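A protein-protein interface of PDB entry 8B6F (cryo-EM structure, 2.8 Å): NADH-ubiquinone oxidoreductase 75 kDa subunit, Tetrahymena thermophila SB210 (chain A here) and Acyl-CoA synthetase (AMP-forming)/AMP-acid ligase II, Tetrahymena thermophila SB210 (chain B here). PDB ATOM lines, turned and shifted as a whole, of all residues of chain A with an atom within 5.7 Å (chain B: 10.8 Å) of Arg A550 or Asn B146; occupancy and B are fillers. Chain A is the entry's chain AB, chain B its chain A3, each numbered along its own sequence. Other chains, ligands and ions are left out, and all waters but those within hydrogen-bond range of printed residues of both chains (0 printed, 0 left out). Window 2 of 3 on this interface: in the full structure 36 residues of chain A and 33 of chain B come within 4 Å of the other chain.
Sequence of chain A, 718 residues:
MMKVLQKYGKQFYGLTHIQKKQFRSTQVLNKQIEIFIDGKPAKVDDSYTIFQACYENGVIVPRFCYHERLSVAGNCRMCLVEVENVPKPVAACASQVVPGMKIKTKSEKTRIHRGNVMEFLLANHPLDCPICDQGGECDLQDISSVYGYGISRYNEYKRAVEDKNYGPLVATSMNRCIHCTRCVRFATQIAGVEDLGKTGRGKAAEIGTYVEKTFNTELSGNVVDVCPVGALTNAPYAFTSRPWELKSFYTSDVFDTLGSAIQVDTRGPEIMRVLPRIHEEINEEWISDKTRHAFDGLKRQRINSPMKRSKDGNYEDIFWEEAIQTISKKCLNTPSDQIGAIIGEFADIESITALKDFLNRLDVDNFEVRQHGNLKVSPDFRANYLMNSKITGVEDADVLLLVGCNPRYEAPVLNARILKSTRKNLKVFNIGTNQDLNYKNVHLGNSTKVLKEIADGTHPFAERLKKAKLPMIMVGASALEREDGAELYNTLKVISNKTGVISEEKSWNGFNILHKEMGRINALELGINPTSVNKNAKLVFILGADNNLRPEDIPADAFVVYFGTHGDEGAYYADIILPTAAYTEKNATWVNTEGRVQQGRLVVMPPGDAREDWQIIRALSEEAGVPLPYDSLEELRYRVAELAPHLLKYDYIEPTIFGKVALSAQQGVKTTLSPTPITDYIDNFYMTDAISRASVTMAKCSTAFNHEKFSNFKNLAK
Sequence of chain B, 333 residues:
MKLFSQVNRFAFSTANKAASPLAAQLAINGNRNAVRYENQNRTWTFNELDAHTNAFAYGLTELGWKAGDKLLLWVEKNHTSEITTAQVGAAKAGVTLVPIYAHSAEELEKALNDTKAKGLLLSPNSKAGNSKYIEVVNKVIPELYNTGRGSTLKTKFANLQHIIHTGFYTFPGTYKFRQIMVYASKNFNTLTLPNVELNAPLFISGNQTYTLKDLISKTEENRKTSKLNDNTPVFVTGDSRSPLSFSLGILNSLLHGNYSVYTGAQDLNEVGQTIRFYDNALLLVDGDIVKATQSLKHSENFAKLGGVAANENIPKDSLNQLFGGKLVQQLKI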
ATOM      1  N   GLN A 371      10.872   4.268   0.814  1.00  0.00           N
ATOM      2  CA  GLN A 371      11.129   4.550  -0.589  1.00  0.00           C
ATOM      3  C   GLN A 371      11.276   6.035  -0.883  1.00  0.00           C
ATOM      4  O   GLN A 371      11.734   6.389  -1.974  1.00  0.00           O
ATOM      5  CB  GLN A 371      10.005   3.964  -1.461  1.00  0.00           C
ATOM      6  CG  GLN A 371       8.600   4.477  -1.135  1.00  0.00           C
ATOM      7  CD  GLN A 371       8.313   5.847  -1.725  1.00  0.00           C
ATOM      8  OE1 GLN A 371       8.982   6.288  -2.659  1.00  0.00           O
ATOM      9  NE2 GLN A 371       7.311   6.527  -1.178  1.00  0.00           N
ATOM     10  N   HIS A 372      10.902   6.907   0.055  1.00  0.00           N
ATOM     11  CA  HIS A 372      10.971   8.341  -0.199  1.00  0.00           C
ATOM     12  C   HIS A 372      12.416   8.808  -0.339  1.00  0.00           C
ATOM     13  O   HIS A 372      12.766   9.491  -1.309  1.00  0.00           O
ATOM     14  CB  HIS A 372      10.264   9.101   0.923  1.00  0.00           C
ATOM     15  CG  HIS A 372       9.934  10.518   0.575  1.00  0.00           C
ATOM     16  ND1 HIS A 372      10.719  11.583   0.963  1.00  0.00           N
ATOM     17  CD2 HIS A 372       8.904  11.048  -0.127  1.00  0.00           C
ATOM     18  CE1 HIS A 372      10.188  12.706   0.516  1.00  0.00           C
ATOM     19  NE2 HIS A 372       9.085  12.409  -0.149  1.00  0.00           N
ATOM     20  N   ASN A 548      12.651  10.355   9.512  1.00  0.00           N
ATOM     21  CA  ASN A 548      12.112  10.191   8.168  1.00  0.00           C
ATOM     22  C   ASN A 548      10.934   9.223   8.133  1.00  0.00           C
ATOM     23  O   ASN A 548      10.364   9.015   7.055  1.00  0.00           O
ATOM     24  CB  ASN A 548      13.172   9.706   7.165  1.00  0.00           C
ATOM     25  CG  ASN A 548      14.438  10.538   7.209  1.00  0.00           C
ATOM     26  OD1 ASN A 548      14.399  11.732   7.503  1.00  0.00           O
ATOM     27  ND2 ASN A 548      15.570   9.909   6.917  1.00  0.00           N
ATOM     28  N   LEU A 549      10.550   8.625   9.257  1.00  0.00           N
ATOM     29  CA  LEU A 549       9.407   7.723   9.262  1.00  0.00           C
ATOM     30  C   LEU A 549       8.118   8.487   8.993  1.00  0.00           C
ATOM     31  O   LEU A 549       7.884   9.562   9.552  1.00  0.00           O
ATOM     32  CB  LEU A 549       9.304   6.992  10.600  1.00  0.00           C
ATOM     33  CG  LEU A 549      10.390   5.963  10.917  1.00  0.00           C
ATOM     34  CD1 LEU A 549      10.138   5.356  12.283  1.00  0.00           C
ATOM     35  CD2 LEU A 549      10.458   4.873   9.857  1.00  0.00           C
ATOM     36  N   ARG A 550       7.282   7.925   8.134  1.00  0.00           N
ATOM     37  CA  ARG A 550       5.967   8.464   7.835  1.00  0.00           C
ATOM     38  C   ARG A 550       4.991   7.306   7.712  1.00  0.00           C
ATOM     39  O   ARG A 550       5.393   6.179   7.406  1.00  0.00           O
ATOM     40  CB  ARG A 550       5.966   9.294   6.545  1.00  0.00           C
ATOM     41  CG  ARG A 550       6.872  10.514   6.603  1.00  0.00           C
ATOM     42  CD  ARG A 550       6.728  11.387   5.362  1.00  0.00           C
ATOM     43  NE  ARG A 550       7.124  10.686   4.145  1.00  0.00           N
ATOM     44  CZ  ARG A 550       6.300   9.993   3.369  1.00  0.00           C
ATOM     45  NH1 ARG A 550       5.012   9.878   3.652  1.00  0.00           N
ATOM     46  NH2 ARG A 550       6.782   9.397   2.283  1.00  0.00           N
ATOM     47  N   PRO A 551       3.700   7.552   7.945  1.00  0.00           N
ATOM     48  CA  PRO A 551       2.727   6.451   7.857  1.00  0.00           C
ATOM     49  C   PRO A 551       2.722   5.756   6.509  1.00  0.00           C
ATOM     50  O   PRO A 551       2.499   4.540   6.451  1.00  0.00           O
ATOM     51  CB  PRO A 551       1.387   7.146   8.139  1.00  0.00           C
ATOM     52  CG  PRO A 551       1.745   8.372   8.901  1.00  0.00           C
ATOM     53  CD  PRO A 551       3.068   8.814   8.364  1.00  0.00           C
ATOM     54  N   GLU A 552       2.960   6.488   5.420  1.00  0.00           N
ATOM     55  CA  GLU A 552       2.915   5.882   4.094  1.00  0.00           C
ATOM     56  C   GLU A 552       3.973   4.799   3.930  1.00  0.00           C
ATOM     57  O   GLU A 552       3.774   3.850   3.164  1.00  0.00           O
ATOM     58  CB  GLU A 552       3.101   6.957   3.021  1.00  0.00           C
ATOM     59  CG  GLU A 552       2.115   8.116   3.105  1.00  0.00           C
ATOM     60  CD  GLU A 552       0.688   7.700   2.807  1.00  0.00           C
ATOM     61  OE1 GLU A 552       0.461   6.509   2.504  1.00  0.00           O
ATOM     62  OE2 GLU A 552      -0.209   8.567   2.867  1.00  0.00           O
ATOM     63  N   ASP A 553       5.101   4.921   4.634  1.00  0.00           N
ATOM     64  CA  ASP A 553       6.181   3.949   4.480  1.00  0.00           C
ATOM     65  C   ASP A 553       5.780   2.571   4.996  1.00  0.00           C
ATOM     66  O   ASP A 553       6.195   1.551   4.435  1.00  0.00           O
ATOM     67  CB  ASP A 553       7.432   4.445   5.203  1.00  0.00           C
ATOM     68  CG  ASP A 553       7.963   5.742   4.626  1.00  0.00           C
ATOM     69  OD1 ASP A 553       7.262   6.769   4.727  1.00  0.00           O
ATOM     70  OD2 ASP A 553       9.083   5.736   4.072  1.00  0.00           O
ATOM     71  N   ILE A 554       4.988   2.516   6.059  1.00  0.00           N
ATOM     72  CA  ILE A 554       4.573   1.258   6.672  1.00  0.00           C
ATOM     73  C   ILE A 554       3.195   0.897   6.126  1.00  0.00           C
ATOM     74  O   ILE A 554       2.232   1.638   6.376  1.00  0.00           O
ATOM     75  CB  ILE A 554       4.545   1.362   8.205  1.00  0.00           C
ATOM     76  CG1 ILE A 554       5.934   1.719   8.749  1.00  0.00           C
ATOM     77  CG2 ILE A 554       4.045   0.060   8.825  1.00  0.00           C
ATOM     78  CD1 ILE A 554       7.008   0.678   8.480  1.00  0.00           C
ATOM     79  N   TYR A 573       4.495   3.111  15.436  1.00  0.00           N
ATOM     80  CA  TYR A 573       4.311   2.247  14.280  1.00  0.00           C
ATOM     81  C   TYR A 573       4.510   0.777  14.612  1.00  0.00           C
ATOM     82  O   TYR A 573       4.324  -0.072  13.734  1.00  0.00           O
ATOM     83  CB  TYR A 573       5.285   2.634  13.160  1.00  0.00           C
ATOM     84  CG  TYR A 573       5.282   4.097  12.784  1.00  0.00           C
ATOM     85  CD1 TYR A 573       5.984   5.028  13.538  1.00  0.00           C
ATOM     86  CD2 TYR A 573       4.608   4.542  11.656  1.00  0.00           C
ATOM     87  CE1 TYR A 573       5.997   6.364  13.192  1.00  0.00           C
ATOM     88  CE2 TYR A 573       4.613   5.876  11.302  1.00  0.00           C
ATOM     89  CZ  TYR A 573       5.311   6.781  12.074  1.00  0.00           C
ATOM     90  OH  TYR A 573       5.323   8.111  11.728  1.00  0.00           O
ATOM     91  N   VAL B 137      -1.965  25.361   2.147  1.00  0.00           N
ATOM     92  CA  VAL B 137      -1.233  25.058   0.920  1.00  0.00           C
ATOM     93  C   VAL B 137      -1.190  23.556   0.688  1.00  0.00           C
ATOM     94  O   VAL B 137      -1.413  23.076  -0.430  1.00  0.00           O
ATOM     95  CB  VAL B 137       0.181  25.661   0.979  1.00  0.00           C
ATOM     96  CG1 VAL B 137       1.011  25.226  -0.221  1.00  0.00           C
ATOM     97  CG2 VAL B 137       0.097  27.161   1.012  1.00  0.00           C
ATOM     98  N   ASN B 138      -0.903  22.788   1.739  1.00  0.00           N
ATOM     99  CA  ASN B 138      -0.877  21.338   1.600  1.00  0.00           C
ATOM    100  C   ASN B 138      -2.249  20.808   1.210  1.00  0.00           C
ATOM    101  O   ASN B 138      -2.359  19.902   0.377  1.00  0.00           O
ATOM    102  CB  ASN B 138      -0.404  20.698   2.905  1.00  0.00           C
ATOM    103  CG  ASN B 138       1.020  21.076   3.256  1.00  0.00           C
ATOM    104  OD1 ASN B 138       1.839  21.342   2.377  1.00  0.00           O
ATOM    105  ND2 ASN B 138       1.323  21.106   4.549  1.00  0.00           N
ATOM    106  N   LYS B 139      -3.309  21.358   1.806  1.00  0.00           N
ATOM    107  CA  LYS B 139      -4.655  20.917   1.461  1.00  0.00           C
ATOM    108  C   LYS B 139      -4.966  21.197  -0.004  1.00  0.00           C
ATOM    109  O   LYS B 139      -5.544  20.352  -0.696  1.00  0.00           O
ATOM    110  CB  LYS B 139      -5.672  21.609   2.368  1.00  0.00           C
ATOM    111  CG  LYS B 139      -7.100  21.096   2.228  1.00  0.00           C
ATOM    112  CD  LYS B 139      -7.223  19.616   2.580  1.00  0.00           C
ATOM    113  CE  LYS B 139      -6.700  19.307   3.979  1.00  0.00           C
ATOM    114  NZ  LYS B 139      -7.276  20.210   5.014  1.00  0.00           N
ATOM    115  N   ILE B 141      -2.794  21.499  -2.398  1.00  0.00           N
ATOM    116  CA  ILE B 141      -1.878  20.714  -3.221  1.00  0.00           C
ATOM    117  C   ILE B 141      -1.412  19.505  -2.420  1.00  0.00           C
ATOM    118  O   ILE B 141      -0.307  19.524  -1.859  1.00  0.00           O
ATOM    119  CB  ILE B 141      -0.680  21.559  -3.682  1.00  0.00           C
ATOM    120  CG1 ILE B 141      -1.167  22.864  -4.317  1.00  0.00           C
ATOM    121  CG2 ILE B 141       0.174  20.764  -4.665  1.00  0.00           C
ATOM    122  CD1 ILE B 141      -0.057  23.817  -4.702  1.00  0.00           C
ATOM    123  N   PRO B 142      -2.207  18.438  -2.336  1.00  0.00           N
ATOM    124  CA  PRO B 142      -1.772  17.266  -1.560  1.00  0.00           C
ATOM    125  C   PRO B 142      -0.524  16.603  -2.109  1.00  0.00           C
ATOM    126  O   PRO B 142       0.133  15.853  -1.377  1.00  0.00           O
ATOM    127  CB  PRO B 142      -2.985  16.328  -1.629  1.00  0.00           C
ATOM    128  CG  PRO B 142      -3.724  16.747  -2.852  1.00  0.00           C
ATOM    129  CD  PRO B 142      -3.522  18.228  -2.965  1.00  0.00           C
ATOM    130  N   GLU B 143      -0.174  16.850  -3.373  1.00  0.00           N
ATOM    131  CA  GLU B 143       1.000  16.211  -3.957  1.00  0.00           C
ATOM    132  C   GLU B 143       2.284  16.610  -3.246  1.00  0.00           C
ATOM    133  O   GLU B 143       3.271  15.869  -3.315  1.00  0.00           O
ATOM    134  CB  GLU B 143       1.107  16.555  -5.444  1.00  0.00           C
ATOM    135  CG  GLU B 143       0.063  15.881  -6.324  1.00  0.00           C
ATOM    136  CD  GLU B 143      -1.330  16.450  -6.132  1.00  0.00           C
ATOM    137  OE1 GLU B 143      -1.487  17.382  -5.317  1.00  0.00           O
ATOM    138  OE2 GLU B 143      -2.267  15.965  -6.798  1.00  0.00           O
ATOM    139  N   LEU B 144       2.298  17.757  -2.566  1.00  0.00           N
ATOM    140  CA  LEU B 144       3.517  18.198  -1.895  1.00  0.00           C
ATOM    141  C   LEU B 144       3.939  17.219  -0.809  1.00  0.00           C
ATOM    142  O   LEU B 144       5.137  17.023  -0.581  1.00  0.00           O
ATOM    143  CB  LEU B 144       3.315  19.590  -1.298  1.00  0.00           C
ATOM    144  CG  LEU B 144       2.917  20.699  -2.273  1.00  0.00           C
ATOM    145  CD1 LEU B 144       2.757  22.017  -1.535  1.00  0.00           C
ATOM    146  CD2 LEU B 144       3.928  20.836  -3.399  1.00  0.00           C
ATOM    147  N   TYR B 145       2.973  16.596  -0.132  1.00  0.00           N
ATOM    148  CA  TYR B 145       3.303  15.727   0.992  1.00  0.00           C
ATOM    149  C   TYR B 145       4.186  14.565   0.555  1.00  0.00           C
ATOM    150  O   TYR B 145       5.151  14.217   1.245  1.00  0.00           O
ATOM    151  CB  TYR B 145       2.022  15.207   1.641  1.00  0.00           C
ATOM    152  CG  TYR B 145       2.267  14.314   2.833  1.00  0.00           C
ATOM    153  CD1 TYR B 145       2.437  14.847   4.105  1.00  0.00           C
ATOM    154  CD2 TYR B 145       2.329  12.934   2.686  1.00  0.00           C
ATOM    155  CE1 TYR B 145       2.662  14.031   5.196  1.00  0.00           C
ATOM    156  CE2 TYR B 145       2.552  12.109   3.771  1.00  0.00           C
ATOM    157  CZ  TYR B 145       2.718  12.663   5.023  1.00  0.00           C
ATOM    158  OH  TYR B 145       2.941  11.844   6.104  1.00  0.00           O
ATOM    159  N   ASN B 146       3.872  13.953  -0.585  1.00  0.00           N
ATOM    160  CA  ASN B 146       4.605  12.796  -1.076  1.00  0.00           C
ATOM    161  C   ASN B 146       5.611  13.154  -2.164  1.00  0.00           C
ATOM    162  O   ASN B 146       6.186  12.254  -2.783  1.00  0.00           O
ATOM    163  CB  ASN B 146       3.624  11.741  -1.594  1.00  0.00           C
ATOM    164  CG  ASN B 146       4.282  10.394  -1.815  1.00  0.00           C
ATOM    165  OD1 ASN B 146       4.671  10.054  -2.933  1.00  0.00           O
ATOM    166  ND2 ASN B 146       4.416   9.618  -0.744  1.00  0.00           N
ATOM    167  N   THR B 147       5.837  14.441  -2.413  1.00  0.00           N
ATOM    168  CA  THR B 147       6.802  14.841  -3.427  1.00  0.00           C
ATOM    169  C   THR B 147       8.205  14.407  -3.022  1.00  0.00           C
ATOM    170  O   THR B 147       8.598  14.516  -1.858  1.00  0.00           O
ATOM    171  CB  THR B 147       6.760  16.357  -3.636  1.00  0.00           C
ATOM    172  OG1 THR B 147       5.460  16.745  -4.099  1.00  0.00           O
ATOM    173  CG2 THR B 147       7.808  16.799  -4.655  1.00  0.00           C
ATOM    174  N   GLY B 148       8.962  13.915  -3.998  1.00  0.00           N
ATOM    175  CA  GLY B 148      10.305  13.451  -3.726  1.00  0.00           C
ATOM    176  C   GLY B 148      11.246  14.581  -3.358  1.00  0.00           C
ATOM    177  O   GLY B 148      11.020  15.753  -3.660  1.00  0.00           O
ATOM    178  N   ARG B 149      12.329  14.209  -2.681  1.00  0.00           N
ATOM    179  CA  ARG B 149      13.341  15.176  -2.279  1.00  0.00           C
ATOM    180  C   ARG B 149      14.167  15.581  -3.492  1.00  0.00           C
ATOM    181  O   ARG B 149      14.866  14.751  -4.082  1.00  0.00           O
ATOM    182  CB  ARG B 149      14.231  14.586  -1.188  1.00  0.00           C
ATOM    183  CG  ARG B 149      13.477  14.231   0.086  1.00  0.00           C
ATOM    184  CD  ARG B 149      14.368  13.527   1.100  1.00  0.00           C
ATOM    185  NE  ARG B 149      13.643  13.218   2.327  1.00  0.00           N
ATOM    186  CZ  ARG B 149      14.141  12.523   3.342  1.00  0.00           C
ATOM    187  NH1 ARG B 149      15.372  12.042   3.313  1.00  0.00           N
ATOM    188  NH2 ARG B 149      13.384  12.307   4.413  1.00  0.00           N
ATOM    189  N   GLY B 150      14.091  16.856  -3.862  1.00  0.00           N
ATOM    190  CA  GLY B 150      14.758  17.319  -5.061  1.00  0.00           C
ATOM    191  C   GLY B 150      14.012  17.032  -6.343  1.00  0.00           C
ATOM    192  O   GLY B 150      14.636  16.939  -7.405  1.00  0.00           O
ATOM    193  N   SER B 151      12.693  16.882  -6.277  1.00  0.00           N
ATOM    194  CA  SER B 151      11.870  16.580  -7.438  1.00  0.00           C
ATOM    195  C   SER B 151      10.996  17.781  -7.774  1.00  0.00           C
ATOM    196  O   SER B 151      10.502  18.471  -6.878  1.00  0.00           O
ATOM    197  CB  SER B 151      10.986  15.358  -7.178  1.00  0.00           C
ATOM    198  OG  SER B 151      10.321  14.946  -8.359  1.00  0.00           O
ATOM    199  N   THR B 152      10.808  18.025  -9.068  1.00  0.00           N
ATOM    200  CA  THR B 152       9.952  19.118  -9.503  1.00  0.00           C
ATOM    201  C   THR B 152       8.494  18.825  -9.168  1.00  0.00           C
ATOM    202  O   THR B 152       8.079  17.669  -9.055  1.00  0.00           O
ATOM    203  CB  THR B 152      10.102  19.355 -11.006  1.00  0.00           C
ATOM    204  OG1 THR B 152       9.781  18.152 -11.717  1.00  0.00           O
ATOM    205  CG2 THR B 152      11.525  19.782 -11.341  1.00  0.00           C
ATOM    206  N   LEU B 153       7.715  19.891  -9.010  1.00  0.00           N
ATOM    207  CA  LEU B 153       6.317  19.754  -8.627  1.00  0.00           C
ATOM    208  C   LEU B 153       5.465  19.410  -9.841  1.00  0.00           C
ATOM    209  O   LEU B 153       5.516  20.099 -10.863  1.00  0.00           O
ATOM    210  CB  LEU B 153       5.812  21.045  -7.982  1.00  0.00           C
ATOM    211  CG  LEU B 153       6.547  21.516  -6.724  1.00  0.00           C
ATOM    212  CD1 LEU B 153       5.928  22.802  -6.201  1.00  0.00           C
ATOM    213  CD2 LEU B 153       6.547  20.441  -5.648  1.00  0.00           C
ATOM    214  N   LYS B 154       4.686  18.339  -9.723  1.00  0.00           N
ATOM    215  CA  LYS B 154       3.715  17.934 -10.736  1.00  0.00           C
ATOM    216  C   LYS B 154       2.332  18.152 -10.126  1.00  0.00           C
ATOM    217  O   LYS B 154       1.753  17.250  -9.521  1.00  0.00           O
ATOM    218  CB  LYS B 154       3.931  16.482 -11.158  1.00  0.00           C
ATOM    219  CG  LYS B 154       2.937  15.971 -12.197  1.00  0.00           C
ATOM    220  CD  LYS B 154       2.949  16.803 -13.477  1.00  0.00           C
ATOM    221  CE  LYS B 154       4.311  16.794 -14.160  1.00  0.00           C
ATOM    222  NZ  LYS B 154       4.780  15.414 -14.473  1.00  0.00           N
ATOM    223  N   THR B 170      11.122  23.137   7.704  1.00  0.00           N
ATOM    224  CA  THR B 170      11.058  22.800   6.291  1.00  0.00           C
ATOM    225  C   THR B 170       9.965  21.765   6.065  1.00  0.00           C
ATOM    226  O   THR B 170       9.728  20.896   6.908  1.00  0.00           O
ATOM    227  CB  THR B 170      12.401  22.256   5.777  1.00  0.00           C
ATOM    228  OG1 THR B 170      12.371  22.181   4.346  1.00  0.00           O
ATOM    229  CG2 THR B 170      12.673  20.865   6.329  1.00  0.00           C
ATOM    230  N   PHE B 171       9.301  21.869   4.920  1.00  0.00           N
ATOM    231  CA  PHE B 171       8.231  20.958   4.551  1.00  0.00           C
ATOM    232  C   PHE B 171       8.483  20.420   3.150  1.00  0.00           C
ATOM    233  O   PHE B 171       9.108  21.094   2.326  1.00  0.00           O
ATOM    234  CB  PHE B 171       6.867  21.661   4.595  1.00  0.00           C
ATOM    235  CG  PHE B 171       6.644  22.463   5.843  1.00  0.00           C
ATOM    236  CD1 PHE B 171       6.246  21.845   7.018  1.00  0.00           C
ATOM    237  CD2 PHE B 171       6.829  23.834   5.843  1.00  0.00           C
ATOM    238  CE1 PHE B 171       6.039  22.581   8.169  1.00  0.00           C
ATOM    239  CE2 PHE B 171       6.625  24.577   6.990  1.00  0.00           C
ATOM    240  CZ  PHE B 171       6.229  23.949   8.155  1.00  0.00           C
ATOM    241  N   PRO B 172       8.012  19.209   2.854  1.00  0.00           N
ATOM    242  CA  PRO B 172       8.236  18.649   1.516  1.00  0.00           C
ATOM    243  C   PRO B 172       7.562  19.491   0.443  1.00  0.00           C
ATOM    244  O   PRO B 172       6.481  20.046   0.650  1.00  0.00           O
ATOM    245  CB  PRO B 172       7.624  17.247   1.610  1.00  0.00           C
ATOM    246  CG  PRO B 172       6.636  17.336   2.717  1.00  0.00           C
ATOM    247  CD  PRO B 172       7.210  18.311   3.701  1.00  0.00           C
ATOM    248  N   GLY B 173       8.214  19.580  -0.715  1.00  0.00           N
ATOM    249  CA  GLY B 173       7.702  20.380  -1.807  1.00  0.00           C
ATOM    250  C   GLY B 173       7.867  21.871  -1.634  1.00  0.00           C
ATOM    251  O   GLY B 173       7.303  22.635  -2.424  1.00  0.00           O
ATOM    252  N   THR B 174       8.619  22.310  -0.627  1.00  0.00           N
ATOM    253  CA  THR B 174       8.803  23.724  -0.342  1.00  0.00           C
ATOM    254  C   THR B 174      10.277  23.987  -0.064  1.00  0.00           C
ATOM    255  O   THR B 174      11.022  23.091   0.339  1.00  0.00           O
ATOM    256  CB  THR B 174       7.951  24.173   0.855  1.00  0.00           C
ATOM    257  OG1 THR B 174       6.612  23.686   0.703  1.00  0.00           O
ATOM    258  CG2 THR B 174       7.917  25.690   0.957  1.00  0.00           C
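NE2 of His A372 touches O of Asn B146, 3.9 Å away.
His A372 touches Gly B148 (NE2 to CA, 3.9 Å).
His A372 touches Arg B149.
Tyr B145 touches Arg A550 (CE2 to NH1, 3.3 Å).
Arg A550 touches Asn B146.
CD of Pro A551 touches OH of Tyr B145 (3.8 Å).
The backbone carbonyl oxygen of Thr B147 is in hydrogen-bond range of a ring nitrogen (NE2) of His A372 (2.8 Å).
NH2 of Arg B149 is in hydrogen-bond range of OD1 of Asn A548.
Of the 22 printed residues of chain B, 5 touch a printed residue of chain A.
Hydrophobic or aromatic side chains of chain B that line the printed part of chain A: Tyr B145.
Of the 10 printed residues of chain A, 4 touch a printed residue of chain B.
Hydrophobic or aromatic side chains of chain A within 4 Å of the printed part of chain B: His A372 and Pro A551.
Among the printed residues, 8 pairs touch across the chains.
Among the printed residues, no Asp or Glu carboxylate lies within 4 Å of a Lys or Arg side-chain nitrogen of the other chain.
No residue of chain B comes within 4 Å of Leu A549.
Arg A550 touches just these residues of chain B: Tyr B145 and Asn B146.
Pro A551 touches just one residue of chain B: Tyr B145.
No residue of chain B comes within 4 Å of Glu A552.
No residue of chain B comes within 4 Å of Ile A554.
Leu B144 touches none of the printed residues of chain A.
Asn B146 touches just these residues of chain A: His A372 (3.9 Å) and Arg A550 (3.8 Å).
Printed residues of chain A within 4 Å of Thr B147: His A372.
Of the printed residues of chain A, Arg B149 touches His A372 (3.6 Å) and Asn A548 (3.3 Å).
Thr B174 touches none of the printed residues of chain A.
The nearest printed residue of chain B that does not touch His A372 is Tyr B145 (4.5 Å).
The guanidinium group (NH2) of Arg A550 is in salt-bridge range of the side-chain carboxylate (OD1) of Asp A553 (3.6 Å).
The side-chain hydroxyl (OG1) of Thr B147 sits at hydrogen-bond distance from the backbone carbonyl oxygen (O) of Glu B143 (2.5 Å).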
